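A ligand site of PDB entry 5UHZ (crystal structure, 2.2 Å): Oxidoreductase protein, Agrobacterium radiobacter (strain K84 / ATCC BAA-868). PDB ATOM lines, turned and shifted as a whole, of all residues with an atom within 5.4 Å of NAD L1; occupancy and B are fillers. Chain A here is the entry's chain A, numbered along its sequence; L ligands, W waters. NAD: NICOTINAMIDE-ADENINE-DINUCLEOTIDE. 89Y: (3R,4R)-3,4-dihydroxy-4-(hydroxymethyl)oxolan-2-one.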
ATOM      1  N   ILE A  11     -24.660 -13.943 -21.124  1.00  0.00           N
ATOM      2  CA  ILE A  11     -23.243 -14.213 -21.283  1.00  0.00           C
ATOM      3  C   ILE A  11     -22.456 -12.916 -21.053  1.00  0.00           C
ATOM      4  O   ILE A  11     -22.589 -11.967 -21.840  1.00  0.00           O
ATOM      5  CB  ILE A  11     -22.936 -14.782 -22.680  1.00  0.00           C
ATOM      6  CG1 ILE A  11     -23.662 -16.118 -22.870  1.00  0.00           C
ATOM      7  CG2 ILE A  11     -21.422 -14.934 -22.881  1.00  0.00           C
ATOM      8  CD1 ILE A  11     -23.545 -16.711 -24.262  1.00  0.00           C
ATOM      9  N   GLY A  12     -21.642 -12.886 -20.008  1.00  0.00           N
ATOM     10  CA  GLY A  12     -20.835 -11.722 -19.648  1.00  0.00           C
ATOM     11  C   GLY A  12     -21.428 -11.025 -18.435  1.00  0.00           C
ATOM     12  O   GLY A  12     -22.223 -10.100 -18.592  1.00  0.00           O
ATOM     13  N   CYS A  13     -21.022 -11.463 -17.246  1.00  0.00           N
ATOM     14  CA  CYS A  13     -21.573 -10.995 -15.967  1.00  0.00           C
ATOM     15  C   CYS A  13     -20.770  -9.833 -15.408  1.00  0.00           C
ATOM     16  O   CYS A  13     -20.292  -9.872 -14.278  1.00  0.00           O
ATOM     17  CB  CYS A  13     -21.578 -12.144 -14.962  1.00  0.00           C
ATOM     18  SG  CYS A  13     -22.683 -13.489 -15.424  1.00  0.00           S
ATOM     19  N   GLY A  14     -20.643  -8.781 -16.216  1.00  0.00           N
ATOM     20  CA  GLY A  14     -19.776  -7.677 -15.875  1.00  0.00           C
ATOM     21  C   GLY A  14     -20.478  -6.555 -15.156  1.00  0.00           C
ATOM     22  O   GLY A  14     -21.529  -6.757 -14.546  1.00  0.00           O
ATOM     23  N   PHE A  15     -19.880  -5.378 -15.250  1.00  0.00           N
ATOM     24  CA  PHE A  15     -20.345  -4.154 -14.582  1.00  0.00           C
ATOM     25  C   PHE A  15     -21.788  -3.835 -15.004  1.00  0.00           C
ATOM     26  O   PHE A  15     -22.682  -3.787 -14.158  1.00  0.00           O
ATOM     27  CB  PHE A  15     -19.337  -3.002 -14.863  1.00  0.00           C
ATOM     28  CG  PHE A  15     -19.892  -1.606 -14.710  1.00  0.00           C
ATOM     29  CD1 PHE A  15     -20.409  -0.930 -15.828  1.00  0.00           C
ATOM     30  CD2 PHE A  15     -19.847  -0.943 -13.479  1.00  0.00           C
ATOM     31  CE1 PHE A  15     -20.907   0.375 -15.702  1.00  0.00           C
ATOM     32  CE2 PHE A  15     -20.346   0.351 -13.363  1.00  0.00           C
ATOM     33  CZ  PHE A  15     -20.873   1.008 -14.472  1.00  0.00           C
ATOM     34  N   PHE A  16     -22.002  -3.692 -16.303  1.00  0.00           N
ATOM     35  CA  PHE A  16     -23.311  -3.321 -16.840  1.00  0.00           C
ATOM     36  C   PHE A  16     -24.328  -4.470 -16.867  1.00  0.00           C
ATOM     37  O   PHE A  16     -25.531  -4.227 -16.861  1.00  0.00           O
ATOM     38  CB  PHE A  16     -23.169  -2.690 -18.224  1.00  0.00           C
ATOM     39  CG  PHE A  16     -24.367  -1.863 -18.626  1.00  0.00           C
ATOM     40  CD1 PHE A  16     -24.591  -0.614 -18.053  1.00  0.00           C
ATOM     41  CD2 PHE A  16     -25.280  -2.324 -19.563  1.00  0.00           C
ATOM     42  CE1 PHE A  16     -25.681   0.156 -18.416  1.00  0.00           C
ATOM     43  CE2 PHE A  16     -26.375  -1.563 -19.929  1.00  0.00           C
ATOM     44  CZ  PHE A  16     -26.576  -0.318 -19.350  1.00  0.00           C
ATOM     45  N   ALA A  17     -23.860  -5.717 -16.902  1.00  0.00           N
ATOM     46  CA  ALA A  17     -24.777  -6.879 -16.854  1.00  0.00           C
ATOM     47  C   ALA A  17     -25.677  -6.867 -15.628  1.00  0.00           C
ATOM     48  O   ALA A  17     -26.809  -7.354 -15.692  1.00  0.00           O
ATOM     49  CB  ALA A  17     -23.994  -8.185 -16.899  1.00  0.00           C
ATOM     50  N   CYS A  36     -23.318 -16.990 -17.679  1.00  0.00           N
ATOM     51  CA  CYS A  36     -22.005 -17.441 -18.099  1.00  0.00           C
ATOM     52  C   CYS A  36     -20.974 -16.324 -18.030  1.00  0.00           C
ATOM     53  O   CYS A  36     -21.239 -15.192 -18.437  1.00  0.00           O
ATOM     54  CB  CYS A  36     -22.075 -17.986 -19.524  1.00  0.00           C
ATOM     55  SG  CYS A  36     -20.455 -18.395 -20.219  1.00  0.00           S
ATOM     56  N   ASP A  37     -19.783 -16.657 -17.524  1.00  0.00           N
ATOM     57  CA  ASP A  37     -18.637 -15.776 -17.547  1.00  0.00           C
ATOM     58  C   ASP A  37     -17.322 -16.578 -17.391  1.00  0.00           C
ATOM     59  O   ASP A  37     -17.264 -17.535 -16.619  1.00  0.00           O
ATOM     60  CB  ASP A  37     -18.764 -14.722 -16.436  1.00  0.00           C
ATOM     61  CG  ASP A  37     -17.874 -13.519 -16.663  1.00  0.00           C
ATOM     62  OD1 ASP A  37     -16.654 -13.695 -16.870  1.00  0.00           O
ATOM     63  OD2 ASP A  37     -18.394 -12.395 -16.639  1.00  0.00           O
ATOM     64  N   ARG A  38     -16.288 -16.183 -18.130  1.00  0.00           N
ATOM     65  CA  ARG A  38     -14.922 -16.735 -17.977  1.00  0.00           C
ATOM     66  C   ARG A  38     -14.311 -16.490 -16.586  1.00  0.00           C
ATOM     67  O   ARG A  38     -13.474 -17.261 -16.143  1.00  0.00           O
ATOM     68  CB  ARG A  38     -13.977 -16.127 -19.013  1.00  0.00           C
ATOM     69  CG  ARG A  38     -14.201 -16.608 -20.438  1.00  0.00           C
ATOM     70  CD  ARG A  38     -13.502 -15.702 -21.427  1.00  0.00           C
ATOM     71  NE  ARG A  38     -13.389 -16.308 -22.756  1.00  0.00           N
ATOM     72  CZ  ARG A  38     -12.983 -15.681 -23.861  1.00  0.00           C
ATOM     73  NH1 ARG A  38     -12.639 -14.383 -23.826  1.00  0.00           N
ATOM     74  NH2 ARG A  38     -12.929 -16.342 -25.021  1.00  0.00           N
ATOM     75  N   ASP A  39     -14.700 -15.390 -15.962  1.00  0.00           N
ATOM     76  CA  ASP A  39     -14.192 -14.969 -14.658  1.00  0.00           C
ATOM     77  C   ASP A  39     -15.090 -15.570 -13.576  1.00  0.00           C
ATOM     78  O   ASP A  39     -16.237 -15.163 -13.452  1.00  0.00           O
ATOM     79  CB  ASP A  39     -14.206 -13.424 -14.609  1.00  0.00           C
ATOM     80  CG  ASP A  39     -13.521 -12.852 -13.384  1.00  0.00           C
ATOM     81  OD1 ASP A  39     -13.182 -13.597 -12.443  1.00  0.00           O
ATOM     82  OD2 ASP A  39     -13.358 -11.616 -13.354  1.00  0.00           O
ATOM     83  N   ARG A  42     -16.884 -13.118 -11.025  1.00  0.00           N
ATOM     84  CA  ARG A  42     -18.064 -12.437 -11.572  1.00  0.00           C
ATOM     85  C   ARG A  42     -19.268 -13.361 -11.707  1.00  0.00           C
ATOM     86  O   ARG A  42     -20.400 -12.964 -11.395  1.00  0.00           O
ATOM     87  CB  ARG A  42     -17.748 -11.815 -12.941  1.00  0.00           C
ATOM     88  CG  ARG A  42     -16.743 -10.662 -12.898  1.00  0.00           C
ATOM     89  CD  ARG A  42     -17.189  -9.528 -11.984  1.00  0.00           C
ATOM     90  NE  ARG A  42     -18.546  -9.055 -12.277  1.00  0.00           N
ATOM     91  CZ  ARG A  42     -19.181  -8.118 -11.583  1.00  0.00           C
ATOM     92  NH1 ARG A  42     -18.620  -7.526 -10.540  1.00  0.00           N
ATOM     93  NH2 ARG A  42     -20.423  -7.765 -11.942  1.00  0.00           N
ATOM     94  N   ALA A  59     -19.172 -20.232 -22.745  1.00  0.00           N
ATOM     95  CA  ALA A  59     -20.405 -20.177 -23.534  1.00  0.00           C
ATOM     96  C   ALA A  59     -20.690 -21.455 -24.345  1.00  0.00           C
ATOM     97  O   ALA A  59     -21.854 -21.810 -24.547  1.00  0.00           O
ATOM     98  CB  ALA A  59     -20.397 -18.964 -24.463  1.00  0.00           C
ATOM     99  N   ALA A  74     -23.698  -9.664 -22.981  1.00  0.00           N
ATOM    100  CA  ALA A  74     -23.260  -8.449 -22.309  1.00  0.00           C
ATOM    101  C   ALA A  74     -21.747  -8.385 -22.118  1.00  0.00           C
ATOM    102  O   ALA A  74     -21.262  -7.693 -21.214  1.00  0.00           O
ATOM    103  CB  ALA A  74     -23.985  -8.325 -20.969  1.00  0.00           C
ATOM    104  N   THR A  75     -20.992  -9.090 -22.963  1.00  0.00           N
ATOM    105  CA  THR A  75     -19.531  -9.060 -22.928  1.00  0.00           C
ATOM    106  C   THR A  75     -19.037  -7.806 -23.651  1.00  0.00           C
ATOM    107  O   THR A  75     -19.802  -7.139 -24.346  1.00  0.00           O
ATOM    108  CB  THR A  75     -18.887 -10.279 -23.643  1.00  0.00           C
ATOM    109  OG1 THR A  75     -19.156 -10.231 -25.049  1.00  0.00           O
ATOM    110  CG2 THR A  75     -19.392 -11.595 -23.076  1.00  0.00           C
ATOM    111  N   THR A  76     -17.737  -7.529 -23.497  1.00  0.00           N
ATOM    112  CA  THR A  76     -17.034  -6.546 -24.325  1.00  0.00           C
ATOM    113  C   THR A  76     -16.946  -7.026 -25.787  1.00  0.00           C
ATOM    114  O   THR A  76     -17.144  -8.206 -26.079  1.00  0.00           O
ATOM    115  CB  THR A  76     -15.620  -6.242 -23.769  1.00  0.00           C
ATOM    116  OG1 THR A  76     -14.907  -7.463 -23.495  1.00  0.00           O
ATOM    117  CG2 THR A  76     -15.714  -5.454 -22.477  1.00  0.00           C
ATOM    118  N   VAL A  77     -16.629  -6.089 -26.684  1.00  0.00           N
ATOM    119  CA  VAL A  77     -16.700  -6.292 -28.144  1.00  0.00           C
ATOM    120  C   VAL A  77     -15.962  -7.514 -28.716  1.00  0.00           C
ATOM    121  O   VAL A  77     -16.424  -8.105 -29.687  1.00  0.00           O
ATOM    122  CB  VAL A  77     -16.243  -5.015 -28.912  1.00  0.00           C
ATOM    123  CG1 VAL A  77     -14.731  -4.808 -28.790  1.00  0.00           C
ATOM    124  CG2 VAL A  77     -16.698  -5.040 -30.362  1.00  0.00           C
ATOM    125  N   SER A  79     -15.662 -10.620 -27.950  1.00  0.00           N
ATOM    126  CA  SER A  79     -16.402 -11.881 -28.016  1.00  0.00           C
ATOM    127  C   SER A  79     -17.686 -11.830 -28.842  1.00  0.00           C
ATOM    128  O   SER A  79     -18.278 -12.879 -29.109  1.00  0.00           O
ATOM    129  CB  SER A  79     -16.760 -12.340 -26.600  1.00  0.00           C
ATOM    130  OG  SER A  79     -15.607 -12.793 -25.921  1.00  0.00           O
ATOM    131  N   HIS A  80     -18.122 -10.644 -29.259  1.00  0.00           N
ATOM    132  CA  HIS A  80     -19.461 -10.491 -29.871  1.00  0.00           C
ATOM    133  C   HIS A  80     -19.658 -11.356 -31.119  1.00  0.00           C
ATOM    134  O   HIS A  80     -20.683 -12.020 -31.243  1.00  0.00           O
ATOM    135  CB  HIS A  80     -19.765  -9.035 -30.200  1.00  0.00           C
ATOM    136  CG  HIS A  80     -19.990  -8.188 -28.991  1.00  0.00           C
ATOM    137  ND1 HIS A  80     -20.130  -6.821 -29.070  1.00  0.00           N
ATOM    138  CD2 HIS A  80     -20.073  -8.505 -27.682  1.00  0.00           C
ATOM    139  CE1 HIS A  80     -20.320  -6.329 -27.860  1.00  0.00           C
ATOM    140  NE2 HIS A  80     -20.287  -7.329 -26.997  1.00  0.00           N
ATOM    141  N   LEU A  83     -19.928 -15.247 -30.185  1.00  0.00           N
ATOM    142  CA  LEU A  83     -21.145 -15.556 -29.410  1.00  0.00           C
ATOM    143  C   LEU A  83     -22.420 -15.471 -30.249  1.00  0.00           C
ATOM    144  O   LEU A  83     -23.295 -16.322 -30.136  1.00  0.00           O
ATOM    145  CB  LEU A  83     -21.239 -14.666 -28.177  1.00  0.00           C
ATOM    146  CG  LEU A  83     -20.124 -14.860 -27.130  1.00  0.00           C
ATOM    147  CD1 LEU A  83     -20.262 -13.818 -26.036  1.00  0.00           C
ATOM    148  CD2 LEU A  83     -20.132 -16.263 -26.549  1.00  0.00           C
ATOM    149  N   GLN A  97     -24.709  -6.540 -26.942  1.00  0.00           N
ATOM    150  CA  GLN A  97     -24.321  -5.198 -26.484  1.00  0.00           C
ATOM    151  C   GLN A  97     -23.542  -4.401 -27.543  1.00  0.00           C
ATOM    152  O   GLN A  97     -22.986  -4.973 -28.485  1.00  0.00           O
ATOM    153  CB  GLN A  97     -23.498  -5.256 -25.177  1.00  0.00           C
ATOM    154  CG  GLN A  97     -24.295  -4.979 -23.908  1.00  0.00           C
ATOM    155  CD  GLN A  97     -24.801  -3.541 -23.803  1.00  0.00           C
ATOM    156  OE1 GLN A  97     -24.421  -2.675 -24.590  1.00  0.00           O
ATOM    157  NE2 GLN A  97     -25.674  -3.298 -22.821  1.00  0.00           N
ATOM    158  N   LYS A  98     -23.537  -3.086 -27.369  1.00  0.00           N
ATOM    159  CA  LYS A  98     -22.691  -2.196 -28.161  1.00  0.00           C
ATOM    160  C   LYS A  98     -21.287  -2.147 -27.545  1.00  0.00           C
ATOM    161  O   LYS A  98     -21.119  -2.541 -26.389  1.00  0.00           O
ATOM    162  CB  LYS A  98     -23.285  -0.787 -28.327  1.00  0.00           C
ATOM    163  CG  LYS A  98     -23.878  -0.094 -27.100  1.00  0.00           C
ATOM    164  CD  LYS A  98     -22.902   0.200 -25.969  1.00  0.00           C
ATOM    165  CE  LYS A  98     -21.764   1.132 -26.397  1.00  0.00           C
ATOM    166  NZ  LYS A  98     -21.081   1.743 -25.220  1.00  0.00           N
ATOM    167  N   PRO A  99     -20.264  -1.750 -28.305  1.00  0.00           N
ATOM    168  CA  PRO A  99     -20.327  -1.653 -29.761  1.00  0.00           C
ATOM    169  C   PRO A  99     -20.558  -3.046 -30.371  1.00  0.00           C
ATOM    170  O   PRO A  99     -19.983  -4.016 -29.911  1.00  0.00           O
ATOM    171  CB  PRO A  99     -18.950  -1.086 -30.152  1.00  0.00           C
ATOM    172  CG  PRO A  99     -18.051  -1.450 -29.036  1.00  0.00           C
ATOM    173  CD  PRO A  99     -18.886  -1.666 -27.804  1.00  0.00           C
ATOM    174  N   HIS A 124     -28.353  -4.206 -28.257  1.00  0.00           N
ATOM    175  CA  HIS A 124     -28.723  -3.470 -27.053  1.00  0.00           C
ATOM    176  C   HIS A 124     -28.184  -2.042 -27.156  1.00  0.00           C
ATOM    177  O   HIS A 124     -27.090  -1.735 -26.693  1.00  0.00           O
ATOM    178  CB  HIS A 124     -28.198  -4.176 -25.797  1.00  0.00           C
ATOM    179  CG  HIS A 124     -28.781  -3.661 -24.525  1.00  0.00           C
ATOM    180  ND1 HIS A 124     -29.492  -4.476 -23.664  1.00  0.00           N
ATOM    181  CD2 HIS A 124     -28.773  -2.429 -23.956  1.00  0.00           C
ATOM    182  CE1 HIS A 124     -29.898  -3.760 -22.619  1.00  0.00           C
ATOM    183  NE2 HIS A 124     -29.477  -2.521 -22.779  1.00  0.00           N
ATOM    184  N   ASN A 126     -29.473   1.378 -26.085  1.00  0.00           N
ATOM    185  CA  ASN A 126     -30.560   1.809 -25.184  1.00  0.00           C
ATOM    186  C   ASN A 126     -30.791   3.323 -25.035  1.00  0.00           C
ATOM    187  O   ASN A 126     -31.828   3.728 -24.481  1.00  0.00           O
ATOM    188  CB  ASN A 126     -30.461   1.118 -23.802  1.00  0.00           C
ATOM    189  CG  ASN A 126     -29.153   1.362 -23.084  1.00  0.00           C
ATOM    190  OD1 ASN A 126     -28.490   2.381 -23.298  1.00  0.00           O
ATOM    191  ND2 ASN A 126     -28.776   0.427 -22.212  1.00  0.00           N
ATOM    192  N   PHE A 127     -29.898   4.160 -25.557  1.00  0.00           N
ATOM    193  CA  PHE A 127     -30.075   5.624 -25.446  1.00  0.00           C
ATOM    194  C   PHE A 127     -31.358   6.134 -26.106  1.00  0.00           C
ATOM    195  O   PHE A 127     -32.026   7.001 -25.533  1.00  0.00           O
ATOM    196  CB  PHE A 127     -28.848   6.376 -25.971  1.00  0.00           C
ATOM    197  CG  PHE A 127     -27.765   6.587 -24.933  1.00  0.00           C
ATOM    198  CD1 PHE A 127     -27.274   5.523 -24.189  1.00  0.00           C
ATOM    199  CD2 PHE A 127     -27.243   7.850 -24.699  1.00  0.00           C
ATOM    200  CE1 PHE A 127     -26.284   5.717 -23.227  1.00  0.00           C
ATOM    201  CE2 PHE A 127     -26.247   8.055 -23.749  1.00  0.00           C
ATOM    202  CZ  PHE A 127     -25.779   6.982 -23.007  1.00  0.00           C
ATOM    203  N   GLY A 164     -15.388   2.888 -13.401  1.00  0.00           N
ATOM    204  CA  GLY A 164     -16.307   1.800 -13.670  1.00  0.00           C
ATOM    205  C   GLY A 164     -15.962   0.980 -14.912  1.00  0.00           C
ATOM    206  O   GLY A 164     -16.248  -0.221 -14.951  1.00  0.00           O
ATOM    207  N   GLN A 165     -15.366   1.627 -15.921  1.00  0.00           N
ATOM    208  CA  GLN A 165     -15.019   0.984 -17.186  1.00  0.00           C
ATOM    209  C   GLN A 165     -13.565   1.292 -17.578  1.00  0.00           C
ATOM    210  O   GLN A 165     -13.329   2.120 -18.460  1.00  0.00           O
ATOM    211  CB  GLN A 165     -15.981   1.449 -18.293  1.00  0.00           C
ATOM    212  CG  GLN A 165     -17.418   0.997 -18.096  1.00  0.00           C
ATOM    213  CD  GLN A 165     -18.403   1.737 -18.977  1.00  0.00           C
ATOM    214  OE1 GLN A 165     -19.152   2.588 -18.510  1.00  0.00           O
ATOM    215  NE2 GLN A 165     -18.420   1.417 -20.273  1.00  0.00           N
ATOM    216  N   TYR A 167     -11.150  -0.213 -19.319  1.00  0.00           N
ATOM    217  CA  TYR A 167     -10.852  -0.394 -20.768  1.00  0.00           C
ATOM    218  C   TYR A 167     -11.003   0.873 -21.647  1.00  0.00           C
ATOM    219  O   TYR A 167     -10.295   1.029 -22.658  1.00  0.00           O
ATOM    220  CB  TYR A 167     -11.690  -1.561 -21.363  1.00  0.00           C
ATOM    221  CG  TYR A 167     -13.198  -1.431 -21.190  1.00  0.00           C
ATOM    222  CD1 TYR A 167     -13.975  -0.710 -22.105  1.00  0.00           C
ATOM    223  CD2 TYR A 167     -13.853  -2.057 -20.115  1.00  0.00           C
ATOM    224  CE1 TYR A 167     -15.355  -0.589 -21.938  1.00  0.00           C
ATOM    225  CE2 TYR A 167     -15.227  -1.928 -19.947  1.00  0.00           C
ATOM    226  CZ  TYR A 167     -15.969  -1.206 -20.862  1.00  0.00           C
ATOM    227  OH  TYR A 167     -17.344  -1.081 -20.679  1.00  0.00           O
ATOM    228  N   ASP A 178     -17.511   4.302 -28.030  1.00  0.00           N
ATOM    229  CA  ASP A 178     -18.130   4.058 -26.723  1.00  0.00           C
ATOM    230  C   ASP A 178     -19.439   4.832 -26.557  1.00  0.00           C
ATOM    231  O   ASP A 178     -20.475   4.248 -26.217  1.00  0.00           O
ATOM    232  CB  ASP A 178     -17.176   4.439 -25.589  1.00  0.00           C
ATOM    233  CG  ASP A 178     -17.831   4.338 -24.225  1.00  0.00           C
ATOM    234  OD1 ASP A 178     -18.492   3.313 -23.947  1.00  0.00           O
ATOM    235  OD2 ASP A 178     -17.679   5.287 -23.416  1.00  0.00           O
ATOM    236  N   HIS A 182     -23.949   6.081 -29.443  1.00  0.00           N
ATOM    237  CA  HIS A 182     -25.293   6.370 -28.935  1.00  0.00           C
ATOM    238  C   HIS A 182     -25.892   7.652 -29.541  1.00  0.00           C
ATOM    239  O   HIS A 182     -27.049   7.682 -29.957  1.00  0.00           O
ATOM    240  CB  HIS A 182     -25.291   6.568 -27.423  1.00  0.00           C
ATOM    241  CG  HIS A 182     -24.931   5.356 -26.630  1.00  0.00           C
ATOM    242  ND1 HIS A 182     -25.652   4.188 -26.677  1.00  0.00           N
ATOM    243  CD2 HIS A 182     -23.961   5.168 -25.701  1.00  0.00           C
ATOM    244  CE1 HIS A 182     -25.123   3.309 -25.845  1.00  0.00           C
ATOM    245  NE2 HIS A 182     -24.093   3.881 -25.247  1.00  0.00           N
ATOM    246  N   ILE A 291     -30.443   5.794 -17.911  1.00  0.00           N
ATOM    247  CA  ILE A 291     -29.886   4.665 -18.658  1.00  0.00           C
ATOM    248  C   ILE A 291     -30.519   3.374 -18.139  1.00  0.00           C
ATOM    249  O   ILE A 291     -31.008   2.556 -18.932  1.00  0.00           O
ATOM    250  CB  ILE A 291     -28.344   4.602 -18.569  1.00  0.00           C
ATOM    251  CG1 ILE A 291     -27.721   5.816 -19.279  1.00  0.00           C
ATOM    252  CG2 ILE A 291     -27.811   3.300 -19.159  1.00  0.00           C
ATOM    253  CD1 ILE A 291     -26.235   5.979 -19.066  1.00  0.00           C
HETATM  254  PA  NAD L   1     -16.937  -5.702 -18.037  1.00  0.00           P
HETATM  255  O1A NAD L   1     -15.476  -5.966 -18.328  1.00  0.00           O
HETATM  256  O2A NAD L   1     -17.341  -5.165 -16.691  1.00  0.00           O
HETATM  257  O5B NAD L   1     -17.743  -7.063 -18.255  1.00  0.00           O
HETATM  258  C5B NAD L   1     -17.519  -7.967 -19.341  1.00  0.00           C
HETATM  259  C4B NAD L   1     -17.626  -9.373 -18.781  1.00  0.00           C
HETATM  260  O4B NAD L   1     -17.701 -10.304 -19.851  1.00  0.00           O
HETATM  261  C3B NAD L   1     -16.417  -9.759 -17.937  1.00  0.00           C
HETATM  262  O3B NAD L   1     -16.858 -10.213 -16.657  1.00  0.00           O
HETATM  263  C2B NAD L   1     -15.716 -10.875 -18.721  1.00  0.00           C
HETATM  264  O2B NAD L   1     -15.140 -11.874 -17.879  1.00  0.00           O
HETATM  265  C1B NAD L   1     -16.843 -11.423 -19.581  1.00  0.00           C
HETATM  266  N9A NAD L   1     -16.482 -12.017 -20.884  1.00  0.00           N
HETATM  267  C8A NAD L   1     -15.777 -11.443 -21.887  1.00  0.00           C
HETATM  268  N7A NAD L   1     -15.689 -12.289 -22.945  1.00  0.00           N
HETATM  269  C5A NAD L   1     -16.350 -13.421 -22.631  1.00  0.00           C
HETATM  270  C6A NAD L   1     -16.644 -14.725 -23.280  1.00  0.00           C
HETATM  271  N6A NAD L   1     -16.211 -15.010 -24.534  1.00  0.00           N
HETATM  272  N1A NAD L   1     -17.376 -15.627 -22.590  1.00  0.00           N
HETATM  273  C2A NAD L   1     -17.836 -15.387 -21.333  1.00  0.00           C
HETATM  274  N3A NAD L   1     -17.593 -14.219 -20.692  1.00  0.00           N
HETATM  275  C4A NAD L   1     -16.876 -13.224 -21.275  1.00  0.00           C
HETATM  276  O3  NAD L   1     -17.502  -4.757 -19.210  1.00  0.00           O
HETATM  277  PN  NAD L   1     -18.814  -3.820 -19.005  1.00  0.00           P
HETATM  278  O1N NAD L   1     -18.371  -2.497 -18.429  1.00  0.00           O
HETATM  279  O2N NAD L   1     -19.868  -4.635 -18.304  1.00  0.00           O
HETATM  280  O5D NAD L   1     -19.263  -3.539 -20.516  1.00  0.00           O
HETATM  281  C5D NAD L   1     -19.635  -4.613 -21.370  1.00  0.00           C
HETATM  282  C4D NAD L   1     -20.291  -4.057 -22.614  1.00  0.00           C
HETATM  283  O4D NAD L   1     -21.409  -3.242 -22.243  1.00  0.00           O
HETATM  284  C3D NAD L   1     -19.340  -3.181 -23.427  1.00  0.00           C
HETATM  285  O3D NAD L   1     -19.352  -3.607 -24.798  1.00  0.00           O
HETATM  286  C2D NAD L   1     -19.878  -1.760 -23.267  1.00  0.00           C
HETATM  287  O2D NAD L   1     -19.730  -0.988 -24.464  1.00  0.00           O
HETATM  288  C1D NAD L   1     -21.348  -1.985 -22.917  1.00  0.00           C
HETATM  289  N1N NAD L   1     -22.004  -0.949 -22.084  1.00  0.00           N
HETATM  290  C2N NAD L   1     -23.211  -0.510 -22.486  1.00  0.00           C
HETATM  291  C3N NAD L   1     -23.928   0.454 -21.782  1.00  0.00           C
HETATM  292  C7N NAD L   1     -25.269   0.902 -22.296  1.00  0.00           C
HETATM  293  O7N NAD L   1     -26.025   0.072 -22.790  1.00  0.00           O
HETATM  294  N7N NAD L   1     -25.634   2.180 -22.218  1.00  0.00           N
HETATM  295  C4N NAD L   1     -23.362   0.971 -20.607  1.00  0.00           C
HETATM  296  C5N NAD L   1     -22.113   0.500 -20.192  1.00  0.00           C
HETATM  297  C6N NAD L   1     -21.443  -0.466 -20.955  1.00  0.00           C
HETATM  298  O2  89Y L   2     -20.147   2.815 -21.919  1.00  0.00           O
HETATM  299  C2  89Y L   2     -20.943   3.993 -22.057  1.00  0.00           C
HETATM  300  C1  89Y L   2     -22.353   3.668 -22.405  1.00  0.00           C
HETATM  301  O1  89Y L   2     -22.680   2.841 -23.241  1.00  0.00           O
HETATM  302  O4  89Y L   2     -23.280   4.456 -21.628  1.00  0.00           O
HETATM  303  C4  89Y L   2     -22.541   5.352 -20.783  1.00  0.00           C
HETATM  304  C3  89Y L   2     -21.123   4.772 -20.750  1.00  0.00           C
HETATM  305  O3  89Y L   2     -21.110   3.864 -19.633  1.00  0.00           O
HETATM  306  C5  89Y L   2     -20.029   5.813 -20.506  1.00  0.00           C
HETATM  307  O5  89Y L   2     -19.543   6.416 -21.723  1.00  0.00           O
HETATM  308  O   HOH W   1     -16.475  -3.554 -25.697  1.00  0.00           O
HETATM  309  O   HOH W   2     -15.985  -2.448 -16.427  1.00  0.00           O
HETATM  310  O   HOH W   3     -15.279 -10.123 -24.812  1.00  0.00           O
HETATM  311  O   HOH W   4     -17.125 -18.305 -23.128  1.00  0.00           O
HETATM  312  O   HOH W   5     -17.691   0.778 -24.356  1.00  0.00           O
HETATM  313  O   HOH W   6     -21.306  -6.873 -18.503  1.00  0.00           O
HETATM  314  O   HOH W   7     -26.819   0.546 -25.230  1.00  0.00           O
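Water W7 lies within hydrogen-bond range of O7N of NAD L1 (2.6 Å), O of His 124 (2.7 Å) and N of Asn 126 (2.9 Å).
Water W5 lies within hydrogen-bond range of OD1 of Asp 178 and O2D of NAD L1.
Water W4 bridges N1A of NAD L1 (2.7 Å) and N of Ala 59 (2.8 Å).
Water W3 lies within hydrogen-bond range of a nitrogen (N7A) of NAD L1 (2.9 Å), the side-chain hydroxyl (OG) of Ser 79 (2.9 Å) and the backbone carbonyl oxygen (O) of Thr 76 (3.0 Å).
Water W1 lies within hydrogen-bond range of N of Val 77 and O3D of NAD L1.
Water W2 lies within hydrogen-bond range of the backbone carbonyl oxygen of Gly 164 (2.7 Å) and an oxygen (O2A) of NAD L1 (3.0 Å).
N7N of NAD L1 lies close to O1 of 89Y L2, 3.2 Å away.
The side-chain carboxylate (OD1) of Asp 37 sits at hydrogen-bond distance from an oxygen (O2B) of NAD L1 (2.6 Å).
O of Lys 98 is in hydrogen-bond range of O3D of NAD L1 (2.6 Å).
The side-chain amino group (NZ) of Lys 98 is in hydrogen-bond range of an oxygen (O2D) of NAD L1, 3.1 Å away.
The side-chain hydroxyl (OG) of Ser 79 is in hydrogen-bond range of a nitrogen (N6A) of NAD L1 (2.7 Å).
The side-chain amide nitrogen (ND2) of Asn 126 is in hydrogen-bond range of an oxygen (O7N) of NAD L1 (2.8 Å).
The side-chain hydroxyl of Tyr 167 lies within hydrogen-bond range of an oxygen (O1N) of NAD L1, 2.8 Å away.
N of Phe 15 is in hydrogen-bond range of O2A of NAD L1 (2.9 Å).
The backbone NH (N) of Phe 16 is in hydrogen-bond range of an oxygen (O2N) of NAD L1.
NE2 of Gln 97 sits at hydrogen-bond distance from O7N of NAD L1, at 3.4 Å.
The backbone NH (N) of Arg 38 sits at hydrogen-bond distance from a nitrogen (N3A) of NAD L1 (3.5 Å).
An oxygen (O1) of 89Y L2 is in hydrogen-bond range of the side-chain amino group of Lys 98 (2.8 Å).
The side-chain amide oxygen of Gln 165 sits at hydrogen-bond distance from an oxygen (O3) of 89Y L2 (2.6 Å).
NE2 of His 182 is in hydrogen-bond range of O1 of 89Y L2.
OD1 of Asp 178 is in hydrogen-bond range of O2 of 89Y L2.
CG2 of Ile 11 touches C2A of NAD L1 (3.9 Å).
CA of Gly 12 touches O4B of NAD L1 (3.4 Å).
Gly 14 touches NAD L1.
Asp 39 touches NAD L1.
CG of Arg 42 touches O3B of NAD L1, 3.8 Å away.
Ala 74 touches NAD L1.
CG2 of Thr 75 touches C4A of NAD L1 (3.5 Å).
CA of Thr 76 touches O3D of NAD L1, at 3.8 Å.
Pro 99 touches NAD L1.
CD2 of His 124 touches O7N of NAD L1 (3.9 Å).
Phe 127 touches NAD L1.
Gln 165 touches NAD L1 (NE2 to C6N, 3.6 Å).
NE2 of His 182 touches N7N of NAD L1, 3.8 Å away.
CG2 of Ile 291 touches N7N of NAD L1, at 3.9 Å.
The nearest printed residue that does not touch NAD L1 is Cys 13 (4.1 Å).
The backbone NH (N) of Cys 13 sits at hydrogen-bond distance from the side-chain carboxylate (OD2) of Asp 37.
The side-chain hydroxyl of Tyr 167 sits at hydrogen-bond distance from the side-chain amide nitrogen of Gln 165.
NH2 of Arg 42 lies within hydrogen-bond range of O of Gly 14, at 3.0 Å.
ND1 of His 80 sits close to O of Gln 97 (3.5 Å).
The backbone carbonyl oxygen (O) of Cys 36 lies within hydrogen-bond range of the backbone NH (N) of Gly 12.
O of Ile 11 is in hydrogen-bond range of N of Ala 74.
NE2 of His 80 lies close to O of Thr 76 (3.4 Å).
O of Cys 13 lies within hydrogen-bond range of NE of Arg 42, 2.8 Å away.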
